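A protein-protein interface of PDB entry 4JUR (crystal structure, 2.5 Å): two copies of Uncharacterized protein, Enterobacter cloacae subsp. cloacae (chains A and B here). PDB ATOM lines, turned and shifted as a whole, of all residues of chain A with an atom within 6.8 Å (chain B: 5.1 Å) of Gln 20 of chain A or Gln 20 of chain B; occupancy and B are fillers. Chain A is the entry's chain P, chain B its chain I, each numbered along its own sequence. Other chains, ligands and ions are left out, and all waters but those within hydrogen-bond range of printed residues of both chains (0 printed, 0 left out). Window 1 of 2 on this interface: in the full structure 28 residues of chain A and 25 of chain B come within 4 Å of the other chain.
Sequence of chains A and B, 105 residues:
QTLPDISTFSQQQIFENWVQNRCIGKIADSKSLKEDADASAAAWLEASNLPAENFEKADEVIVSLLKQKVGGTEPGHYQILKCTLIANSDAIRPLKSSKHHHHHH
The side-chain sulfur (SG) of Cys 23 of chain A is disulfide-bonded to the side-chain sulfur (SG) of Cys 83 of chain A, 2.1 Å away. O of Asn 17 of chain B sits close to ND2 of Asn 21 of chain B. The side-chain amide oxygen of Gln 20 of chain A sits at hydrogen-bond distance from the side-chain hydroxyl of Thr 84 of chain A (3.1 Å). The side-chain amide oxygen of Gln 20 of chain B is in hydrogen-bond range of the side-chain hydroxyl of Thr 84 of chain B, 3.3 Å away. ND2 of Asn 21 of chain A sits at hydrogen-bond distance from O of Asn 17 of chain A, at 3.1 Å. SG of Cys 83 of chain B lies within hydrogen-bond range of N of Ile 24 of chain B, at 3.6 Å.
The side-chain hydroxyl (OG1) of Thr 84 of chain B sits at hydrogen-bond distance from the side-chain amide nitrogen (ND2) of Asn 21 of chain A (3.4 Å). The side-chain amide nitrogen (NE2) of Gln 20 of chain A lies close to the side-chain amide nitrogen (NE2) of Gln 20 of chain B.
Among the printed residues, merely in contact across the chains: Ile 80 of chain A with Asn 21 of chain B, Asn 21 of chain A with Ile 80 of chain B, Ile 24 of chain A with Ile 80 of chain B, Thr 84 of chain A with Asn 17 of chain B, Ala 37 of chain A with Ile 80 of chain B, Ile 80 of chain A with Ile 24 of chain B, Asn 17 of chain A with Thr 84 of chain B, Thr 84 of chain A with Asn 21 of chain B and Ile 24 of chain A with Ile 24 of chain B.
Of the 23 printed residues of chain A, 7 touch a printed residue of chain B. Printed residues of chain A that touch a printed residue of chain B: Asn 17, Gln 20, Asn 21, Ile 24, Ala 37, Ile 80 and Thr 84. Hydrophobic or aromatic side chains of chain A that line the printed part of chain B: Ile 24, Ala 37 and Ile 80. Among the printed residues, 11 pairs touch across the chains.
Gln 20 of chain B touches just one residue of chain A: Gln 20 (3.3 Å). Of the printed residues of chain A, Asn 21 of chain B touches Ile 80 (3.5 Å) and Thr 84 (3.7 Å). Of the printed residues of chain A, Ile 24 of chain B touches Ile 24 (3.8 Å) and Ile 80 (3.6 Å). Of the printed residues of chain B, Asn 17 of chain A touches Thr 84. Of the printed residues of chain B, Ala 37 of chain A touches Ile 80. The nearest residue of chain A that does not touch Gln 20 of chain B is Thr 84 of chain A (4.4 Å). The nearest printed residue of chain B that does not touch Asn 17 of chain A is Gln 20 of chain B (6.2 Å).
Asn 17 of chain A touches Thr 84 of chain B, and with the chains exchanged Thr 84 of chain A touches Asn 17 of chain B. Asn 21 of chain A touches Ile 80 of chain B, and with the chains exchanged Ile 80 of chain A touches Asn 21 of chain B. Asn 21 of chain A touches Thr 84 of chain B, and with the chains exchanged Thr 84 of chain A touches Asn 21 of chain B. Ile 24 of chain A touches its own counterpart, Ile 24 of chain B. Of the 11 pairs that touch across the chains among the printed residues, 10 have their exchanged pair printed and touching as well.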
ATOM      1  N   PHE A  15     -32.931 -34.918  11.476  1.00  0.00           N
ATOM      2  CA  PHE A  15     -32.463 -35.729  12.604  1.00  0.00           C
ATOM      3  C   PHE A  15     -31.361 -35.045  13.452  1.00  0.00           C
ATOM      4  O   PHE A  15     -31.435 -35.057  14.696  1.00  0.00           O
ATOM      5  CB  PHE A  15     -32.055 -37.135  12.169  1.00  0.00           C
ATOM      6  CG  PHE A  15     -31.900 -38.106  13.309  1.00  0.00           C
ATOM      7  CD1 PHE A  15     -33.023 -38.625  13.959  1.00  0.00           C
ATOM      8  CD2 PHE A  15     -30.644 -38.504  13.739  1.00  0.00           C
ATOM      9  CE1 PHE A  15     -32.889 -39.523  15.013  1.00  0.00           C
ATOM     10  CE2 PHE A  15     -30.502 -39.395  14.796  1.00  0.00           C
ATOM     11  CZ  PHE A  15     -31.620 -39.905  15.430  1.00  0.00           C
ATOM     12  N   GLU A  16     -30.374 -34.426  12.791  1.00  0.00           N
ATOM     13  CA  GLU A  16     -29.248 -33.763  13.481  1.00  0.00           C
ATOM     14  C   GLU A  16     -29.770 -32.640  14.360  1.00  0.00           C
ATOM     15  O   GLU A  16     -29.324 -32.422  15.492  1.00  0.00           O
ATOM     16  CB  GLU A  16     -28.223 -33.197  12.478  1.00  0.00           C
ATOM     17  CG  GLU A  16     -27.541 -34.255  11.600  1.00  0.00           C
ATOM     18  CD  GLU A  16     -27.039 -33.750  10.211  1.00  0.00           C
ATOM     19  OE1 GLU A  16     -27.038 -32.528   9.898  1.00  0.00           O
ATOM     20  OE2 GLU A  16     -26.628 -34.612   9.416  1.00  0.00           O
ATOM     21  N   ASN A  17     -30.746 -31.937  13.822  1.00  0.00           N
ATOM     22  CA  ASN A  17     -31.344 -30.824  14.524  1.00  0.00           C
ATOM     23  C   ASN A  17     -32.227 -31.252  15.698  1.00  0.00           C
ATOM     24  O   ASN A  17     -32.284 -30.556  16.724  1.00  0.00           O
ATOM     25  CB  ASN A  17     -32.074 -29.945  13.520  1.00  0.00           C
ATOM     26  CG  ASN A  17     -31.105 -29.320  12.544  1.00  0.00           C
ATOM     27  OD1 ASN A  17     -30.008 -28.925  12.944  1.00  0.00           O
ATOM     28  ND2 ASN A  17     -31.471 -29.258  11.266  1.00  0.00           N
ATOM     29  N   TRP A  18     -32.883 -32.403  15.560  1.00  0.00           N
ATOM     30  CA  TRP A  18     -33.598 -32.965  16.694  1.00  0.00           C
ATOM     31  C   TRP A  18     -32.599 -33.229  17.816  1.00  0.00           C
ATOM     32  O   TRP A  18     -32.875 -32.924  18.983  1.00  0.00           O
ATOM     33  CB  TRP A  18     -34.306 -34.265  16.331  1.00  0.00           C
ATOM     34  CG  TRP A  18     -35.001 -34.871  17.498  1.00  0.00           C
ATOM     35  CD1 TRP A  18     -36.285 -34.637  17.901  1.00  0.00           C
ATOM     36  CD2 TRP A  18     -34.460 -35.814  18.428  1.00  0.00           C
ATOM     37  NE1 TRP A  18     -36.578 -35.374  19.016  1.00  0.00           N
ATOM     38  CE2 TRP A  18     -35.477 -36.108  19.364  1.00  0.00           C
ATOM     39  CE3 TRP A  18     -33.216 -36.435  18.565  1.00  0.00           C
ATOM     40  CZ2 TRP A  18     -35.289 -36.993  20.417  1.00  0.00           C
ATOM     41  CZ3 TRP A  18     -33.031 -37.315  19.620  1.00  0.00           C
ATOM     42  CH2 TRP A  18     -34.066 -37.584  20.532  1.00  0.00           C
ATOM     43  N   VAL A  19     -31.447 -33.807  17.455  1.00  0.00           N
ATOM     44  CA  VAL A  19     -30.435 -34.158  18.445  1.00  0.00           C
ATOM     45  C   VAL A  19     -29.873 -32.919  19.142  1.00  0.00           C
ATOM     46  O   VAL A  19     -29.796 -32.876  20.362  1.00  0.00           O
ATOM     47  CB  VAL A  19     -29.266 -34.943  17.826  1.00  0.00           C
ATOM     48  CG1 VAL A  19     -28.082 -34.970  18.801  1.00  0.00           C
ATOM     49  CG2 VAL A  19     -29.699 -36.323  17.445  1.00  0.00           C
ATOM     50  N   GLN A  20     -29.471 -31.926  18.348  1.00  0.00           N
ATOM     51  CA  GLN A  20     -28.949 -30.665  18.862  1.00  0.00           C
ATOM     52  C   GLN A  20     -29.957 -29.959  19.771  1.00  0.00           C
ATOM     53  O   GLN A  20     -29.567 -29.420  20.807  1.00  0.00           O
ATOM     54  CB  GLN A  20     -28.549 -29.725  17.710  1.00  0.00           C
ATOM     55  CG  GLN A  20     -28.679 -28.219  18.034  1.00  0.00           C
ATOM     56  CD  GLN A  20     -27.339 -27.531  17.979  1.00  0.00           C
ATOM     57  OE1 GLN A  20     -26.702 -27.494  16.913  1.00  0.00           O
ATOM     58  NE2 GLN A  20     -26.868 -27.004  19.129  1.00  0.00           N
ATOM     59  N   ASN A  21     -31.232 -29.947  19.376  1.00  0.00           N
ATOM     60  CA  ASN A  21     -32.262 -29.217  20.122  1.00  0.00           C
ATOM     61  C   ASN A  21     -32.483 -29.905  21.448  1.00  0.00           C
ATOM     62  O   ASN A  21     -32.550 -29.256  22.519  1.00  0.00           O
ATOM     63  CB  ASN A  21     -33.586 -29.131  19.344  1.00  0.00           C
ATOM     64  CG  ASN A  21     -33.584 -28.026  18.301  1.00  0.00           C
ATOM     65  OD1 ASN A  21     -34.644 -27.522  17.910  1.00  0.00           O
ATOM     66  ND2 ASN A  21     -32.390 -27.634  17.843  1.00  0.00           N
ATOM     67  N   ARG A  22     -32.548 -31.229  21.377  1.00  0.00           N
ATOM     68  CA  ARG A  22     -32.733 -32.007  22.576  1.00  0.00           C
ATOM     69  C   ARG A  22     -31.574 -31.812  23.520  1.00  0.00           C
ATOM     70  O   ARG A  22     -31.762 -31.627  24.718  1.00  0.00           O
ATOM     71  CB  ARG A  22     -32.903 -33.494  22.286  1.00  0.00           C
ATOM     72  CG  ARG A  22     -33.397 -34.187  23.532  1.00  0.00           C
ATOM     73  CD  ARG A  22     -33.945 -35.521  23.260  1.00  0.00           C
ATOM     74  NE  ARG A  22     -34.529 -36.084  24.462  1.00  0.00           N
ATOM     75  CZ  ARG A  22     -35.751 -35.789  24.891  1.00  0.00           C
ATOM     76  NH1 ARG A  22     -36.504 -34.919  24.226  1.00  0.00           N
ATOM     77  NH2 ARG A  22     -36.213 -36.355  25.996  1.00  0.00           N
ATOM     78  N   CYS A  23     -30.375 -31.849  22.961  1.00  0.00           N
ATOM     79  CA  CYS A  23     -29.144 -31.696  23.719  1.00  0.00           C
ATOM     80  C   CYS A  23     -29.086 -30.343  24.446  1.00  0.00           C
ATOM     81  O   CYS A  23     -28.707 -30.282  25.637  1.00  0.00           O
ATOM     82  CB  CYS A  23     -27.934 -31.900  22.785  1.00  0.00           C
ATOM     83  SG  CYS A  23     -26.319 -31.574  23.528  1.00  0.00           S
ATOM     84  N   ILE A  24     -29.470 -29.266  23.750  1.00  0.00           N
ATOM     85  CA  ILE A  24     -29.576 -27.960  24.405  1.00  0.00           C
ATOM     86  C   ILE A  24     -30.532 -28.083  25.591  1.00  0.00           C
ATOM     87  O   ILE A  24     -30.221 -27.632  26.697  1.00  0.00           O
ATOM     88  CB  ILE A  24     -30.097 -26.844  23.476  1.00  0.00           C
ATOM     89  CG1 ILE A  24     -29.107 -26.568  22.343  1.00  0.00           C
ATOM     90  CG2 ILE A  24     -30.314 -25.548  24.264  1.00  0.00           C
ATOM     91  CD1 ILE A  24     -27.803 -26.044  22.845  1.00  0.00           C
ATOM     92  N   GLY A  25     -31.681 -28.718  25.358  1.00  0.00           N
ATOM     93  CA  GLY A  25     -32.583 -29.033  26.449  1.00  0.00           C
ATOM     94  C   GLY A  25     -31.911 -29.671  27.652  1.00  0.00           C
ATOM     95  O   GLY A  25     -32.125 -29.229  28.785  1.00  0.00           O
ATOM     96  N   ALA A  37     -36.695 -26.148  24.248  1.00  0.00           N
ATOM     97  CA  ALA A  37     -35.922 -27.165  23.588  1.00  0.00           C
ATOM     98  C   ALA A  37     -36.799 -28.332  23.208  1.00  0.00           C
ATOM     99  O   ALA A  37     -36.698 -28.844  22.092  1.00  0.00           O
ATOM    100  CB  ALA A  37     -34.842 -27.624  24.483  1.00  0.00           C
ATOM    101  N   ILE A  62     -26.874 -39.257  23.316  1.00  0.00           N
ATOM    102  CA  ILE A  62     -26.680 -37.896  23.805  1.00  0.00           C
ATOM    103  C   ILE A  62     -26.239 -37.902  25.266  1.00  0.00           C
ATOM    104  O   ILE A  62     -25.290 -37.194  25.638  1.00  0.00           O
ATOM    105  CB  ILE A  62     -27.964 -37.061  23.679  1.00  0.00           C
ATOM    106  CG1 ILE A  62     -28.262 -36.750  22.216  1.00  0.00           C
ATOM    107  CG2 ILE A  62     -27.863 -35.777  24.489  1.00  0.00           C
ATOM    108  CD1 ILE A  62     -29.705 -36.372  21.986  1.00  0.00           C
ATOM    109  N   GLN A  79     -20.582 -26.468  26.406  1.00  0.00           N
ATOM    110  CA  GLN A  79     -21.667 -27.405  26.195  1.00  0.00           C
ATOM    111  C   GLN A  79     -22.410 -27.098  24.903  1.00  0.00           C
ATOM    112  O   GLN A  79     -22.811 -28.022  24.207  1.00  0.00           O
ATOM    113  CB  GLN A  79     -22.623 -27.381  27.383  1.00  0.00           C
ATOM    114  CG  GLN A  79     -21.946 -27.600  28.714  1.00  0.00           C
ATOM    115  CD  GLN A  79     -22.184 -28.995  29.275  1.00  0.00           C
ATOM    116  OE1 GLN A  79     -21.723 -30.005  28.725  1.00  0.00           O
ATOM    117  NE2 GLN A  79     -22.916 -29.054  30.384  1.00  0.00           N
ATOM    118  N   ILE A  80     -22.570 -25.809  24.578  1.00  0.00           N
ATOM    119  CA  ILE A  80     -23.268 -25.397  23.364  1.00  0.00           C
ATOM    120  C   ILE A  80     -22.566 -25.957  22.133  1.00  0.00           C
ATOM    121  O   ILE A  80     -23.214 -26.560  21.268  1.00  0.00           O
ATOM    122  CB  ILE A  80     -23.353 -23.864  23.204  1.00  0.00           C
ATOM    123  CG1 ILE A  80     -24.166 -23.225  24.322  1.00  0.00           C
ATOM    124  CG2 ILE A  80     -23.964 -23.506  21.863  1.00  0.00           C
ATOM    125  CD1 ILE A  80     -25.549 -23.728  24.385  1.00  0.00           C
ATOM    126  N   LEU A  81     -21.244 -25.763  22.063  1.00  0.00           N
ATOM    127  CA  LEU A  81     -20.439 -26.348  21.001  1.00  0.00           C
ATOM    128  C   LEU A  81     -20.598 -27.867  21.037  1.00  0.00           C
ATOM    129  O   LEU A  81     -20.822 -28.541  19.995  1.00  0.00           O
ATOM    130  CB  LEU A  81     -18.969 -25.979  21.180  1.00  0.00           C
ATOM    131  CG  LEU A  81     -17.913 -26.766  20.397  1.00  0.00           C
ATOM    132  CD1 LEU A  81     -18.086 -26.603  18.892  1.00  0.00           C
ATOM    133  CD2 LEU A  81     -16.523 -26.346  20.815  1.00  0.00           C
ATOM    134  N   LYS A  82     -20.497 -28.410  22.246  1.00  0.00           N
ATOM    135  CA  LYS A  82     -20.554 -29.853  22.402  1.00  0.00           C
ATOM    136  C   LYS A  82     -21.846 -30.462  21.818  1.00  0.00           C
ATOM    137  O   LYS A  82     -21.818 -31.549  21.260  1.00  0.00           O
ATOM    138  CB  LYS A  82     -20.343 -30.243  23.865  1.00  0.00           C
ATOM    139  CG  LYS A  82     -20.081 -31.725  24.066  1.00  0.00           C
ATOM    140  CD  LYS A  82     -20.379 -32.132  25.487  1.00  0.00           C
ATOM    141  CE  LYS A  82     -19.516 -31.358  26.456  1.00  0.00           C
ATOM    142  NZ  LYS A  82     -19.957 -31.536  27.869  1.00  0.00           N
ATOM    143  N   CYS A  83     -22.966 -29.753  21.923  1.00  0.00           N
ATOM    144  CA  CYS A  83     -24.249 -30.227  21.372  1.00  0.00           C
ATOM    145  C   CYS A  83     -24.250 -30.377  19.862  1.00  0.00           C
ATOM    146  O   CYS A  83     -24.679 -31.409  19.348  1.00  0.00           O
ATOM    147  CB  CYS A  83     -25.398 -29.309  21.782  1.00  0.00           C
ATOM    148  SG  CYS A  83     -25.924 -29.556  23.488  1.00  0.00           S
ATOM    149  N   THR A  84     -23.761 -29.350  19.169  1.00  0.00           N
ATOM    150  CA  THR A  84     -23.539 -29.380  17.717  1.00  0.00           C
ATOM    151  C   THR A  84     -22.591 -30.521  17.316  1.00  0.00           C
ATOM    152  O   THR A  84     -22.786 -31.167  16.282  1.00  0.00           O
ATOM    153  CB  THR A  84     -22.943 -28.038  17.182  1.00  0.00           C
ATOM    154  OG1 THR A  84     -23.768 -26.933  17.568  1.00  0.00           O
ATOM    155  CG2 THR A  84     -22.808 -28.054  15.657  1.00  0.00           C
ATOM    156  N   LEU A  85     -21.570 -30.779  18.133  1.00  0.00           N
ATOM    157  CA  LEU A  85     -20.635 -31.851  17.806  1.00  0.00           C
ATOM    158  C   LEU A  85     -21.325 -33.189  17.938  1.00  0.00           C
ATOM    159  O   LEU A  85     -21.134 -34.107  17.124  1.00  0.00           O
ATOM    160  CB  LEU A  85     -19.398 -31.801  18.691  1.00  0.00           C
ATOM    161  CG  LEU A  85     -18.652 -30.489  18.466  1.00  0.00           C
ATOM    162  CD1 LEU A  85     -17.371 -30.436  19.269  1.00  0.00           C
ATOM    163  CD2 LEU A  85     -18.392 -30.280  16.989  1.00  0.00           C
ATOM    164  N   ILE A  86     -22.129 -33.298  18.981  1.00  0.00           N
ATOM    165  CA  ILE A  86     -22.827 -34.538  19.262  1.00  0.00           C
ATOM    166  C   ILE A  86     -23.795 -34.880  18.115  1.00  0.00           C
ATOM    167  O   ILE A  86     -23.870 -36.037  17.672  1.00  0.00           O
ATOM    168  CB  ILE A  86     -23.533 -34.441  20.616  1.00  0.00           C
ATOM    169  CG1 ILE A  86     -22.502 -34.609  21.727  1.00  0.00           C
ATOM    170  CG2 ILE A  86     -24.616 -35.470  20.735  1.00  0.00           C
ATOM    171  CD1 ILE A  86     -23.058 -34.348  23.117  1.00  0.00           C
ATOM    172  N   ALA A  87     -24.495 -33.863  17.615  1.00  0.00           N
ATOM    173  CA  ALA A  87     -25.433 -34.056  16.513  1.00  0.00           C
ATOM    174  C   ALA A  87     -24.752 -34.541  15.227  1.00  0.00           C
ATOM    175  O   ALA A  87     -25.404 -35.113  14.340  1.00  0.00           O
ATOM    176  CB  ALA A  87     -26.185 -32.780  16.250  1.00  0.00           C
ATOM    177  N   ASN A  88     -23.448 -34.297  15.118  1.00  0.00           N
ATOM    178  CA  ASN A  88     -22.698 -34.640  13.911  1.00  0.00           C
ATOM    179  C   ASN A  88     -21.691 -35.762  14.172  1.00  0.00           C
ATOM    180  O   ASN A  88     -20.832 -36.025  13.346  1.00  0.00           O
ATOM    181  CB  ASN A  88     -21.997 -33.403  13.304  1.00  0.00           C
ATOM    182  CG  ASN A  88     -22.983 -32.343  12.793  1.00  0.00           C
ATOM    183  OD1 ASN A  88     -23.445 -32.407  11.651  1.00  0.00           O
ATOM    184  ND2 ASN A  88     -23.301 -31.364  13.639  1.00  0.00           N
ATOM    185  N   GLU B  16     -22.779 -21.206   9.687  1.00  0.00           N
ATOM    186  CA  GLU B  16     -24.093 -21.537  10.229  1.00  0.00           C
ATOM    187  C   GLU B  16     -24.011 -21.843  11.722  1.00  0.00           C
ATOM    188  O   GLU B  16     -24.798 -21.312  12.487  1.00  0.00           O
ATOM    189  CB  GLU B  16     -24.727 -22.733   9.508  1.00  0.00           C
ATOM    190  CG  GLU B  16     -25.203 -22.445   8.120  1.00  0.00           C
ATOM    191  CD  GLU B  16     -25.222 -23.693   7.248  1.00  0.00           C
ATOM    192  OE1 GLU B  16     -25.355 -24.808   7.799  1.00  0.00           O
ATOM    193  OE2 GLU B  16     -25.086 -23.559   6.007  1.00  0.00           O
ATOM    194  N   ASN B  17     -23.080 -22.699  12.133  1.00  0.00           N
ATOM    195  CA  ASN B  17     -22.909 -23.017  13.556  1.00  0.00           C
ATOM    196  C   ASN B  17     -22.513 -21.800  14.408  1.00  0.00           C
ATOM    197  O   ASN B  17     -22.977 -21.661  15.533  1.00  0.00           O
ATOM    198  CB  ASN B  17     -21.937 -24.192  13.784  1.00  0.00           C
ATOM    199  CG  ASN B  17     -22.409 -25.492  13.102  1.00  0.00           C
ATOM    200  OD1 ASN B  17     -23.597 -25.796  13.078  1.00  0.00           O
ATOM    201  ND2 ASN B  17     -21.469 -26.249  12.545  1.00  0.00           N
ATOM    202  N   TRP B  18     -21.675 -20.913  13.878  1.00  0.00           N
ATOM    203  CA  TRP B  18     -21.429 -19.653  14.573  1.00  0.00           C
ATOM    204  C   TRP B  18     -22.760 -18.904  14.812  1.00  0.00           C
ATOM    205  O   TRP B  18     -23.036 -18.446  15.932  1.00  0.00           O
ATOM    206  CB  TRP B  18     -20.464 -18.748  13.806  1.00  0.00           C
ATOM    207  CG  TRP B  18     -20.163 -17.508  14.586  1.00  0.00           C
ATOM    208  CD1 TRP B  18     -19.149 -17.337  15.474  1.00  0.00           C
ATOM    209  CD2 TRP B  18     -20.893 -16.275  14.570  1.00  0.00           C
ATOM    210  NE1 TRP B  18     -19.193 -16.081  16.011  1.00  0.00           N
ATOM    211  CE2 TRP B  18     -20.258 -15.405  15.479  1.00  0.00           C
ATOM    212  CE3 TRP B  18     -22.015 -15.819  13.871  1.00  0.00           C
ATOM    213  CZ2 TRP B  18     -20.708 -14.107  15.717  1.00  0.00           C
ATOM    214  CZ3 TRP B  18     -22.468 -14.535  14.112  1.00  0.00           C
ATOM    215  CH2 TRP B  18     -21.812 -13.690  15.027  1.00  0.00           C
ATOM    216  N   VAL B  19     -23.583 -18.787  13.773  1.00  0.00           N
ATOM    217  CA  VAL B  19     -24.881 -18.131  13.922  1.00  0.00           C
ATOM    218  C   VAL B  19     -25.789 -18.840  14.952  1.00  0.00           C
ATOM    219  O   VAL B  19     -26.365 -18.200  15.851  1.00  0.00           O
ATOM    220  CB  VAL B  19     -25.625 -17.991  12.568  1.00  0.00           C
ATOM    221  CG1 VAL B  19     -27.033 -17.503  12.795  1.00  0.00           C
ATOM    222  CG2 VAL B  19     -24.870 -17.057  11.626  1.00  0.00           C
ATOM    223  N   GLN B  20     -25.898 -20.157  14.846  1.00  0.00           N
ATOM    224  CA  GLN B  20     -26.753 -20.888  15.766  1.00  0.00           C
ATOM    225  C   GLN B  20     -26.300 -20.691  17.224  1.00  0.00           C
ATOM    226  O   GLN B  20     -27.114 -20.390  18.113  1.00  0.00           O
ATOM    227  CB  GLN B  20     -26.784 -22.362  15.410  1.00  0.00           C
ATOM    228  CG  GLN B  20     -28.086 -23.053  15.785  1.00  0.00           C
ATOM    229  CD  GLN B  20     -27.968 -23.917  17.038  1.00  0.00           C
ATOM    230  OE1 GLN B  20     -28.890 -24.681  17.357  1.00  0.00           O
ATOM    231  NE2 GLN B  20     -26.835 -23.800  17.763  1.00  0.00           N
ATOM    232  N   ASN B  21     -24.999 -20.847  17.457  1.00  0.00           N
ATOM    233  CA  ASN B  21     -24.441 -20.695  18.791  1.00  0.00           C
ATOM    234  C   ASN B  21     -24.708 -19.293  19.346  1.00  0.00           C
ATOM    235  O   ASN B  21     -25.299 -19.151  20.416  1.00  0.00           O
ATOM    236  CB  ASN B  21     -22.945 -21.038  18.807  1.00  0.00           C
ATOM    237  CG  ASN B  21     -22.676 -22.553  18.683  1.00  0.00           C
ATOM    238  OD1 ASN B  21     -21.543 -22.992  18.841  1.00  0.00           O
ATOM    239  ND2 ASN B  21     -23.715 -23.342  18.402  1.00  0.00           N
ATOM    240  N   ARG B  22     -24.307 -18.263  18.605  1.00  0.00           N
ATOM    241  CA  ARG B  22     -24.518 -16.912  19.071  1.00  0.00           C
ATOM    242  C   ARG B  22     -25.983 -16.626  19.397  1.00  0.00           C
ATOM    243  O   ARG B  22     -26.294 -15.978  20.410  1.00  0.00           O
ATOM    244  CB  ARG B  22     -23.992 -15.886  18.069  1.00  0.00           C
ATOM    245  CG  ARG B  22     -24.442 -14.476  18.403  1.00  0.00           C
ATOM    246  CD  ARG B  22     -23.399 -13.452  18.093  1.00  0.00           C
ATOM    247  NE  ARG B  22     -22.391 -13.417  19.135  1.00  0.00           N
ATOM    248  CZ  ARG B  22     -21.876 -12.295  19.629  1.00  0.00           C
ATOM    249  NH1 ARG B  22     -22.286 -11.102  19.174  1.00  0.00           N
ATOM    250  NH2 ARG B  22     -20.952 -12.373  20.583  1.00  0.00           N
ATOM    251  N   CYS B  23     -26.875 -17.115  18.541  1.00  0.00           N
ATOM    252  CA  CYS B  23     -28.309 -16.944  18.728  1.00  0.00           C
ATOM    253  C   CYS B  23     -28.737 -17.549  20.078  1.00  0.00           C
ATOM    254  O   CYS B  23     -29.484 -16.925  20.873  1.00  0.00           O
ATOM    255  CB  CYS B  23     -29.063 -17.570  17.536  1.00  0.00           C
ATOM    256  SG  CYS B  23     -30.866 -17.535  17.670  1.00  0.00           S
ATOM    257  N   ILE B  24     -28.224 -18.751  20.357  1.00  0.00           N
ATOM    258  CA  ILE B  24     -28.513 -19.395  21.635  1.00  0.00           C
ATOM    259  C   ILE B  24     -28.011 -18.544  22.803  1.00  0.00           C
ATOM    260  O   ILE B  24     -28.669 -18.457  23.837  1.00  0.00           O
ATOM    261  CB  ILE B  24     -27.991 -20.838  21.697  1.00  0.00           C
ATOM    262  CG1 ILE B  24     -28.985 -21.768  20.997  1.00  0.00           C
ATOM    263  CG2 ILE B  24     -27.817 -21.293  23.132  1.00  0.00           C
ATOM    264  CD1 ILE B  24     -28.377 -23.064  20.536  1.00  0.00           C
ATOM    265  N   ILE B  80     -35.368 -22.129  20.430  1.00  0.00           N
ATOM    266  CA  ILE B  80     -34.253 -22.997  20.074  1.00  0.00           C
ATOM    267  C   ILE B  80     -34.314 -23.462  18.599  1.00  0.00           C
ATOM    268  O   ILE B  80     -33.336 -23.301  17.816  1.00  0.00           O
ATOM    269  CB  ILE B  80     -34.152 -24.137  21.109  1.00  0.00           C
ATOM    270  CG1 ILE B  80     -33.430 -23.590  22.356  1.00  0.00           C
ATOM    271  CG2 ILE B  80     -33.429 -25.348  20.555  1.00  0.00           C
ATOM    272  CD1 ILE B  80     -33.571 -24.449  23.564  1.00  0.00           C
ATOM    273  N   CYS B  83     -33.579 -20.492  16.441  1.00  0.00           N
ATOM    274  CA  CYS B  83     -32.154 -20.271  16.239  1.00  0.00           C
ATOM    275  C   CYS B  83     -31.649 -21.150  15.104  1.00  0.00           C
ATOM    276  O   CYS B  83     -30.905 -20.684  14.224  1.00  0.00           O
ATOM    277  CB  CYS B  83     -31.371 -20.565  17.516  1.00  0.00           C
ATOM    278  SG  CYS B  83     -31.379 -19.225  18.735  1.00  0.00           S
ATOM    279  N   THR B  84     -32.058 -22.418  15.118  1.00  0.00           N
ATOM    280  CA  THR B  84     -31.645 -23.313  14.045  1.00  0.00           C
ATOM    281  C   THR B  84     -32.111 -22.793  12.661  1.00  0.00           C
ATOM    282  O   THR B  84     -31.354 -22.806  11.688  1.00  0.00           O
ATOM    283  CB  THR B  84     -32.122 -24.759  14.297  1.00  0.00           C
ATOM    284  OG1 THR B  84     -31.618 -25.224  15.561  1.00  0.00           O
ATOM    285  CG2 THR B  84     -31.671 -25.701  13.185  1.00  0.00           C
ATOM    286  N   ALA B  87     -30.079 -19.612  11.546  1.00  0.00           N
ATOM    287  CA  ALA B  87     -28.798 -20.056  11.004  1.00  0.00           C
ATOM    288  C   ALA B  87     -28.859 -20.476   9.532  1.00  0.00           C
ATOM    289  O   ALA B  87     -27.893 -20.272   8.791  1.00  0.00           O
ATOM    290  CB  ALA B  87     -28.212 -21.175  11.856  1.00  0.00           C
